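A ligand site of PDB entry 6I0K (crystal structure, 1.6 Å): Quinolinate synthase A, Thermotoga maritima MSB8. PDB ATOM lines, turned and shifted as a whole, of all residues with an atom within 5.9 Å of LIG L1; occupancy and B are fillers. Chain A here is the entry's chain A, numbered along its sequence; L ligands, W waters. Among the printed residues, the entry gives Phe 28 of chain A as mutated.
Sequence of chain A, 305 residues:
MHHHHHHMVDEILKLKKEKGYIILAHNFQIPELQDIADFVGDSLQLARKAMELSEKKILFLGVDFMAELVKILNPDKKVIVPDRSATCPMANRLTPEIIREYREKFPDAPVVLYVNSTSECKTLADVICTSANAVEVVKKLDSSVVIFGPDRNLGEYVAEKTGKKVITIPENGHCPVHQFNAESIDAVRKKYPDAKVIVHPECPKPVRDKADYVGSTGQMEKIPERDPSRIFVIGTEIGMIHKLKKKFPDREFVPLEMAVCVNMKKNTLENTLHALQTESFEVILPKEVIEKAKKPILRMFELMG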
ATOM      1  N   HIS A  26      12.750  22.814  24.948  1.00  0.00           N
ATOM      2  CA  HIS A  26      13.827  21.924  24.460  1.00  0.00           C
ATOM      3  C   HIS A  26      15.122  22.171  25.240  1.00  0.00           C
ATOM      4  O   HIS A  26      15.372  23.301  25.723  1.00  0.00           O
ATOM      5  CB  HIS A  26      14.040  22.101  22.955  1.00  0.00           C
ATOM      6  CG  HIS A  26      14.947  21.056  22.403  1.00  0.00           C
ATOM      7  ND1 HIS A  26      16.297  21.289  22.197  1.00  0.00           N
ATOM      8  CD2 HIS A  26      14.718  19.780  22.023  1.00  0.00           C
ATOM      9  CE1 HIS A  26      16.857  20.203  21.730  1.00  0.00           C
ATOM     10  NE2 HIS A  26      15.910  19.258  21.602  1.00  0.00           N
ATOM     11  N   ASN A  27      15.939  21.123  25.313  1.00  0.00           N
ATOM     12  CA  ASN A  27      17.286  21.153  25.926  1.00  0.00           C
ATOM     13  C   ASN A  27      18.159  22.316  25.396  1.00  0.00           C
ATOM     14  O   ASN A  27      19.074  22.726  26.125  1.00  0.00           O
ATOM     15  CB  ASN A  27      17.960  19.802  25.700  1.00  0.00           C
ATOM     16  CG  ASN A  27      17.330  18.681  26.500  1.00  0.00           C
ATOM     17  OD1 ASN A  27      16.745  18.897  27.562  1.00  0.00           O
ATOM     18  ND2 ASN A  27      17.419  17.457  25.977  1.00  0.00           N
ATOM     19  N   PHE A  28      17.927  22.809  24.172  1.00  0.00           N
ATOM     20  CA  PHE A  28      18.816  23.826  23.538  1.00  0.00           C
ATOM     21  C   PHE A  28      18.307  25.259  23.761  1.00  0.00           C
ATOM     22  O   PHE A  28      18.879  26.198  23.172  1.00  0.00           O
ATOM     23  CB  PHE A  28      18.990  23.534  22.047  1.00  0.00           C
ATOM     24  CG  PHE A  28      19.697  22.242  21.711  1.00  0.00           C
ATOM     25  CD1 PHE A  28      20.365  21.501  22.680  1.00  0.00           C
ATOM     26  CD2 PHE A  28      19.688  21.757  20.416  1.00  0.00           C
ATOM     27  CE1 PHE A  28      21.012  20.319  22.356  1.00  0.00           C
ATOM     28  CE2 PHE A  28      20.335  20.576  20.092  1.00  0.00           C
ATOM     29  CZ  PHE A  28      20.985  19.851  21.067  1.00  0.00           C
ATOM     30  N   GLY A  41      13.200  18.855  27.885  1.00  0.00           N
ATOM     31  CA  GLY A  41      13.699  17.569  27.376  1.00  0.00           C
ATOM     32  C   GLY A  41      13.914  17.591  25.891  1.00  0.00           C
ATOM     33  O   GLY A  41      13.916  18.679  25.302  1.00  0.00           O
ATOM     34  N   ASP A  42      14.104  16.407  25.322  1.00  0.00           N
ATOM     35  CA  ASP A  42      14.273  16.246  23.856  1.00  0.00           C
ATOM     36  C   ASP A  42      12.898  16.277  23.187  1.00  0.00           C
ATOM     37  O   ASP A  42      11.883  16.257  23.899  1.00  0.00           O
ATOM     38  CB  ASP A  42      15.162  15.034  23.539  1.00  0.00           C
ATOM     39  CG  ASP A  42      14.553  13.660  23.764  1.00  0.00           C
ATOM     40  OD1 ASP A  42      13.314  13.546  23.849  1.00  0.00           O
ATOM     41  OD2 ASP A  42      15.341  12.675  23.790  1.00  0.00           O
ATOM     42  N   SER A  43      12.842  16.320  21.846  1.00  0.00           N
ATOM     43  CA  SER A  43      11.575  16.530  21.095  1.00  0.00           C
ATOM     44  C   SER A  43      10.541  15.445  21.456  1.00  0.00           C
ATOM     45  O   SER A  43       9.380  15.799  21.717  1.00  0.00           O
ATOM     46  CB  SER A  43      11.841  16.592  19.609  1.00  0.00           C
ATOM     47  OG  SER A  43      12.288  15.335  19.139  1.00  0.00           O
ATOM     48  N   LEU A  44      10.929  14.180  21.432  1.00  0.00           N
ATOM     49  CA  LEU A  44       9.959  13.075  21.640  1.00  0.00           C
ATOM     50  C   LEU A  44       9.567  13.004  23.122  1.00  0.00           C
ATOM     51  O   LEU A  44       8.394  12.736  23.399  1.00  0.00           O
ATOM     52  CB  LEU A  44      10.557  11.762  21.129  1.00  0.00           C
ATOM     53  CG  LEU A  44       9.608  10.560  21.092  1.00  0.00           C
ATOM     54  CD1 LEU A  44       8.351  10.852  20.275  1.00  0.00           C
ATOM     55  CD2 LEU A  44      10.333   9.352  20.527  1.00  0.00           C
ATOM     56  N   VAL A  63      12.016  24.718  18.140  1.00  0.00           N
ATOM     57  CA  VAL A  63      11.905  25.071  16.692  1.00  0.00           C
ATOM     58  C   VAL A  63      10.683  24.374  16.090  1.00  0.00           C
ATOM     59  O   VAL A  63      10.063  23.499  16.742  1.00  0.00           O
ATOM     60  CB  VAL A  63      13.195  24.778  15.901  1.00  0.00           C
ATOM     61  CG1 VAL A  63      14.358  25.603  16.419  1.00  0.00           C
ATOM     62  CG2 VAL A  63      13.544  23.291  15.863  1.00  0.00           C
ATOM     63  N   PHE A  65       9.659  22.163  13.845  1.00  0.00           N
ATOM     64  CA  PHE A  65       9.370  20.724  13.591  1.00  0.00           C
ATOM     65  C   PHE A  65       8.994  20.058  14.912  1.00  0.00           C
ATOM     66  O   PHE A  65       8.176  19.130  14.901  1.00  0.00           O
ATOM     67  CB  PHE A  65      10.526  19.981  12.910  1.00  0.00           C
ATOM     68  CG  PHE A  65      11.712  19.655  13.786  1.00  0.00           C
ATOM     69  CD1 PHE A  65      11.665  18.635  14.726  1.00  0.00           C
ATOM     70  CD2 PHE A  65      12.891  20.374  13.659  1.00  0.00           C
ATOM     71  CE1 PHE A  65      12.748  18.343  15.520  1.00  0.00           C
ATOM     72  CE2 PHE A  65      13.985  20.079  14.455  1.00  0.00           C
ATOM     73  CZ  PHE A  65      13.918  19.064  15.391  1.00  0.00           C
ATOM     74  N   MET A  66       9.547  20.552  16.029  1.00  0.00           N
ATOM     75  CA  MET A  66       9.267  20.012  17.380  1.00  0.00           C
ATOM     76  C   MET A  66       7.882  20.456  17.842  1.00  0.00           C
ATOM     77  O   MET A  66       7.111  19.641  18.431  1.00  0.00           O
ATOM     78  CB  MET A  66      10.248  20.538  18.414  1.00  0.00           C
ATOM     79  CG  MET A  66      11.669  20.414  18.050  1.00  0.00           C
ATOM     80  SD  MET A  66      12.686  21.022  19.401  1.00  0.00           S
ATOM     81  CE  MET A  66      14.214  20.363  18.733  1.00  0.00           C
ATOM     82  N   CYS A  88      14.594  24.512  11.629  1.00  0.00           N
ATOM     83  CA  CYS A  88      15.843  23.738  11.500  1.00  0.00           C
ATOM     84  C   CYS A  88      16.332  23.854  10.063  1.00  0.00           C
ATOM     85  O   CYS A  88      15.740  23.270   9.164  1.00  0.00           O
ATOM     86  CB  CYS A  88      15.623  22.280  11.896  1.00  0.00           C
ATOM     87  SG  CYS A  88      17.085  21.255  11.587  1.00  0.00           S
ATOM     88  N   TYR A 114      14.631  11.068  10.093  1.00  0.00           N
ATOM     89  CA  TYR A 114      15.042  11.627  11.395  1.00  0.00           C
ATOM     90  C   TYR A 114      13.943  12.623  11.788  1.00  0.00           C
ATOM     91  O   TYR A 114      13.417  13.321  10.907  1.00  0.00           O
ATOM     92  CB  TYR A 114      16.431  12.232  11.225  1.00  0.00           C
ATOM     93  CG  TYR A 114      17.075  12.804  12.462  1.00  0.00           C
ATOM     94  CD1 TYR A 114      16.800  12.314  13.732  1.00  0.00           C
ATOM     95  CD2 TYR A 114      18.007  13.819  12.349  1.00  0.00           C
ATOM     96  CE1 TYR A 114      17.430  12.830  14.856  1.00  0.00           C
ATOM     97  CE2 TYR A 114      18.642  14.354  13.469  1.00  0.00           C
ATOM     98  CZ  TYR A 114      18.336  13.861  14.735  1.00  0.00           C
ATOM     99  OH  TYR A 114      18.941  14.391  15.842  1.00  0.00           O
ATOM    100  N   VAL A 115      13.562  12.621  13.063  1.00  0.00           N
ATOM    101  CA  VAL A 115      12.516  13.513  13.616  1.00  0.00           C
ATOM    102  C   VAL A 115      12.832  14.976  13.273  1.00  0.00           C
ATOM    103  O   VAL A 115      11.880  15.757  13.142  1.00  0.00           O
ATOM    104  CB  VAL A 115      12.337  13.308  15.131  1.00  0.00           C
ATOM    105  CG1 VAL A 115      13.565  13.732  15.930  1.00  0.00           C
ATOM    106  CG2 VAL A 115      11.075  13.998  15.633  1.00  0.00           C
ATOM    107  N   ASN A 116      14.109  15.315  13.150  1.00  0.00           N
ATOM    108  CA  ASN A 116      14.573  16.647  12.688  1.00  0.00           C
ATOM    109  C   ASN A 116      14.325  16.682  11.180  1.00  0.00           C
ATOM    110  O   ASN A 116      15.299  16.527  10.414  1.00  0.00           O
ATOM    111  CB  ASN A 116      16.028  16.925  13.072  1.00  0.00           C
ATOM    112  CG  ASN A 116      16.320  16.803  14.561  1.00  0.00           C
ATOM    113  OD1 ASN A 116      15.643  16.062  15.303  1.00  0.00           O
ATOM    114  ND2 ASN A 116      17.375  17.480  15.021  1.00  0.00           N
ATOM    115  N   THR A 130      14.483   8.931  16.163  1.00  0.00           N
ATOM    116  CA  THR A 130      15.231   9.942  16.971  1.00  0.00           C
ATOM    117  C   THR A 130      16.702   9.565  16.877  1.00  0.00           C
ATOM    118  O   THR A 130      16.989   8.450  16.441  1.00  0.00           O
ATOM    119  CB  THR A 130      14.744   9.974  18.420  1.00  0.00           C
ATOM    120  OG1 THR A 130      15.109   8.731  19.026  1.00  0.00           O
ATOM    121  CG2 THR A 130      13.247  10.173  18.544  1.00  0.00           C
ATOM    122  N   SER A 131      17.616  10.406  17.349  1.00  0.00           N
ATOM    123  CA  SER A 131      19.060  10.057  17.380  1.00  0.00           C
ATOM    124  C   SER A 131      19.296   8.922  18.389  1.00  0.00           C
ATOM    125  O   SER A 131      20.238   8.152  18.179  1.00  0.00           O
ATOM    126  CB  SER A 131      19.949  11.242  17.679  1.00  0.00           C
ATOM    127  OG  SER A 131      19.535  11.883  18.867  1.00  0.00           O
ATOM    128  N   HIS A 178      26.846  20.794  14.992  1.00  0.00           N
ATOM    129  CA  HIS A 178      27.575  19.596  15.483  1.00  0.00           C
ATOM    130  C   HIS A 178      28.869  19.364  14.691  1.00  0.00           C
ATOM    131  O   HIS A 178      29.493  18.317  14.913  1.00  0.00           O
ATOM    132  CB  HIS A 178      26.650  18.368  15.454  1.00  0.00           C
ATOM    133  CG  HIS A 178      25.656  18.384  16.562  1.00  0.00           C
ATOM    134  ND1 HIS A 178      24.373  18.880  16.401  1.00  0.00           N
ATOM    135  CD2 HIS A 178      25.775  18.035  17.857  1.00  0.00           C
ATOM    136  CE1 HIS A 178      23.737  18.809  17.553  1.00  0.00           C
ATOM    137  NE2 HIS A 178      24.573  18.297  18.460  1.00  0.00           N
ATOM    138  N   HIS A 200      27.536  13.896  20.086  1.00  0.00           N
ATOM    139  CA  HIS A 200      26.273  13.553  19.411  1.00  0.00           C
ATOM    140  C   HIS A 200      26.584  12.731  18.163  1.00  0.00           C
ATOM    141  O   HIS A 200      27.582  12.982  17.496  1.00  0.00           O
ATOM    142  CB  HIS A 200      25.496  14.827  19.054  1.00  0.00           C
ATOM    143  CG  HIS A 200      24.034  14.583  18.877  1.00  0.00           C
ATOM    144  ND1 HIS A 200      23.476  14.141  17.678  1.00  0.00           N
ATOM    145  CD2 HIS A 200      23.004  14.746  19.737  1.00  0.00           C
ATOM    146  CE1 HIS A 200      22.172  14.022  17.827  1.00  0.00           C
ATOM    147  NE2 HIS A 200      21.866  14.374  19.084  1.00  0.00           N
ATOM    148  N   GLU A 202      25.300  13.155  15.366  1.00  0.00           N
ATOM    149  CA  GLU A 202      25.265  14.138  14.258  1.00  0.00           C
ATOM    150  C   GLU A 202      26.667  14.709  14.024  1.00  0.00           C
ATOM    151  O   GLU A 202      26.888  15.378  13.001  1.00  0.00           O
ATOM    152  CB  GLU A 202      24.246  15.250  14.526  1.00  0.00           C
ATOM    153  CG  GLU A 202      22.820  14.784  14.326  1.00  0.00           C
ATOM    154  CD  GLU A 202      21.750  15.863  14.367  1.00  0.00           C
ATOM    155  OE1 GLU A 202      21.632  16.653  13.419  1.00  0.00           O
ATOM    156  OE2 GLU A 202      21.022  15.882  15.336  1.00  0.00           O
ATOM    157  N   GLY A 215      26.039   9.722  21.904  1.00  0.00           N
ATOM    158  CA  GLY A 215      24.602   9.590  22.141  1.00  0.00           C
ATOM    159  C   GLY A 215      23.834  10.861  21.909  1.00  0.00           C
ATOM    160  O   GLY A 215      24.454  11.941  21.762  1.00  0.00           O
ATOM    161  N   SER A 216      22.520  10.709  21.899  1.00  0.00           N
ATOM    162  CA  SER A 216      21.509  11.789  21.845  1.00  0.00           C
ATOM    163  C   SER A 216      21.583  12.630  23.121  1.00  0.00           C
ATOM    164  O   SER A 216      22.204  12.185  24.099  1.00  0.00           O
ATOM    165  CB  SER A 216      20.142  11.209  21.685  1.00  0.00           C
ATOM    166  OG  SER A 216      19.732  10.575  22.882  1.00  0.00           O
ATOM    167  N   THR A 217      20.915  13.770  23.152  1.00  0.00           N
ATOM    168  CA  THR A 217      20.883  14.611  24.383  1.00  0.00           C
ATOM    169  C   THR A 217      20.246  13.820  25.539  1.00  0.00           C
ATOM    170  O   THR A 217      20.772  13.895  26.672  1.00  0.00           O
ATOM    171  CB  THR A 217      20.215  15.962  24.158  1.00  0.00           C
ATOM    172  OG1 THR A 217      18.825  15.806  23.862  1.00  0.00           O
ATOM    173  CG2 THR A 217      20.886  16.764  23.065  1.00  0.00           C
ATOM    174  N   GLY A 218      19.147  13.103  25.276  1.00  0.00           N
ATOM    175  CA  GLY A 218      18.488  12.230  26.272  1.00  0.00           C
ATOM    176  C   GLY A 218      19.439  11.168  26.806  1.00  0.00           C
ATOM    177  O   GLY A 218      19.386  10.872  28.017  1.00  0.00           O
ATOM    178  N   THR A 236      27.728  18.819  21.988  1.00  0.00           N
ATOM    179  CA  THR A 236      26.411  19.164  21.409  1.00  0.00           C
ATOM    180  C   THR A 236      26.179  20.657  21.615  1.00  0.00           C
ATOM    181  O   THR A 236      27.114  21.356  22.014  1.00  0.00           O
ATOM    182  CB  THR A 236      25.276  18.267  21.936  1.00  0.00           C
ATOM    183  OG1 THR A 236      24.120  18.461  21.130  1.00  0.00           O
ATOM    184  CG2 THR A 236      24.921  18.545  23.376  1.00  0.00           C
ATOM    185  N   MET A 264      17.354  28.103  17.718  1.00  0.00           N
ATOM    186  CA  MET A 264      16.972  27.786  19.115  1.00  0.00           C
ATOM    187  C   MET A 264      17.040  29.057  19.988  1.00  0.00           C
ATOM    188  O   MET A 264      16.207  29.208  20.897  1.00  0.00           O
ATOM    189  CB  MET A 264      17.890  26.710  19.699  1.00  0.00           C
ATOM    190  CG  MET A 264      17.566  25.307  19.218  1.00  0.00           C
ATOM    191  SD  MET A 264      15.998  24.712  19.886  1.00  0.00           S
ATOM    192  CE  MET A 264      15.995  23.102  19.087  1.00  0.00           C
HETATM  193  O1  LIG L   1      18.107  14.948  21.427  1.00  0.00           O
HETATM  194  C1  LIG L   1      18.852  15.122  20.444  1.00  0.00           C
HETATM  195  O2  LIG L   1      19.909  14.497  20.477  1.00  0.00           O
HETATM  196  C2  LIG L   1      18.518  16.253  19.515  1.00  0.00           C
HETATM  197  C3  LIG L   1      17.203  16.719  19.375  1.00  0.00           C
HETATM  198  C4  LIG L   1      15.996  16.036  19.944  1.00  0.00           C
HETATM  199  O3  LIG L   1      15.178  16.672  20.576  1.00  0.00           O
HETATM  200  O4  LIG L   1      15.805  14.817  19.722  1.00  0.00           O
HETATM  201  C5  LIG L   1      19.525  16.980  18.891  1.00  0.00           C
HETATM  202  C6  LIG L   1      19.251  18.104  18.146  1.00  0.00           C
HETATM  203  C7  LIG L   1      17.945  18.540  18.034  1.00  0.00           C
HETATM  204  C8  LIG L   1      16.935  17.831  18.633  1.00  0.00           C
HETATM  205  S1  LIG L   1      17.476  19.958  17.238  1.00  0.00           S
HETATM  206 FE1  LG2 L   2      21.114  21.355  14.274  1.00  0.00          FE
HETATM  207 FE2  LG2 L   2      19.621  23.559  15.184  1.00  0.00          FE
HETATM  208 FE3  LG2 L   2      18.922  20.961  15.848  1.00  0.00          FE
HETATM  209 FE4  LG2 L   2      18.539  21.802  13.336  1.00  0.00          FE
HETATM  210  S1  LG2 L   2      17.432  22.697  15.123  1.00  0.00           S
HETATM  211  S2  LG2 L   2      19.435  19.724  14.028  1.00  0.00           S
HETATM  212  S3  LG2 L   2      20.397  23.262  12.991  1.00  0.00           S
HETATM  213  S4  LG2 L   2      20.938  22.014  16.434  1.00  0.00           S
HETATM  214  O   HOH W   1      13.592  13.293  20.464  1.00  0.00           O
HETATM  215  O   HOH W   2      17.314  13.243  18.067  1.00  0.00           O
HETATM  216  O   HOH W   3      17.643  12.781  22.687  1.00  0.00           O
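The side-chain amide nitrogen (ND2) of Asn 116 sits close to a sulfur (S1) of LIG L1, at 3.3 Å. OG1 of Thr 217 lies within hydrogen-bond range of O1 of LIG L1 (2.7 Å). An oxygen (O2) of LIG L1 lies within hydrogen-bond range of the side-chain hydroxyl (OG) of Ser 131, 3.1 Å away. The backbone NH (N) of Ser 43 lies within hydrogen-bond range of an oxygen (O3) of LIG L1 (2.7 Å). The side-chain amide nitrogen of Asn 116 lies close to a sulfur (S2) of LG2 L2 (3.2 Å). The backbone NH (N) of Thr 217 lies within hydrogen-bond range of an oxygen (O2) of LIG L1 (2.9 Å). NE2 of His 26 is in hydrogen-bond range of O3 of LIG L1, 2.9 Å away. OG of Ser 43 sits close to O3 of LIG L1 (3.5 Å). An oxygen (O2) of LIG L1 is in hydrogen-bond range of a ring nitrogen (NE2) of His 200 (2.4 Å). An iron atom (FE4) of LG2 L2 is bound by the side-chain sulfur (SG) of Cys 88 (2.3 Å).
A sulfur (S1) of LIG L1 is bound to an iron atom (FE3) of LG2 L2, at 2.2 Å.
A ring nitrogen (ND1) of His 26 is in hydrogen-bond range of the backbone NH of Phe 28 (3.0 Å). The side-chain carboxylate (OD1) of Asp 42 lies close to the backbone NH (N) of Leu 44. The side-chain hydroxyl (OG1) of Thr 217 is in hydrogen-bond range of the side-chain amide nitrogen (ND2) of Asn 27, at 3.0 Å. The side-chain carboxylate (OE2) of Glu 202 is in hydrogen-bond range of the side-chain hydroxyl (OH) of Tyr 114 (2.6 Å). NE2 of His 200 sits at hydrogen-bond distance from OG of Ser 131 (3.4 Å). ND1 of His 200 is in hydrogen-bond range of N of Glu 202, 3.1 Å away.
Residues that only touch LIG L1: Phe 28 (3.3 Å), Asp 42 (3.4 Å), Met 66 (3.6 Å), Glu 202 (3.996 Å), Ser 216 (3.4 Å) and Met 264 (3.9 Å). Hydrophobic or aromatic side chains that line LIG L1: His 26, Phe 28, Met 66, His 200 and Met 264. The nearest printed residue that does not touch LIG L1 is Tyr 114 (4.04 Å).
Water W3 lies within hydrogen-bond range of an oxygen (O1) of LIG L1 (2.5 Å), the side-chain carboxylate (OD2) of Asp 42 (2.6 Å), the backbone NH (N) of Gly 218 (3.0 Å), the side-chain hydroxyl (OG) of Ser 216 (3.0 Å) and the backbone NH (N) of Thr 217 (3.4 Å). Water W2 lies within hydrogen-bond range of OG of Ser 131 (2.7 Å), O4 of LIG L1 (2.7 Å) and OH of Tyr 114 (3.0 Å). Water W1 lies within hydrogen-bond range of the side-chain hydroxyl of Ser 43 (2.8 Å), an oxygen (O4) of LIG L1 (2.8 Å), the backbone NH of Leu 44 (3.0 Å) and the side-chain carboxylate of Asp 42 (3.4 Å).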
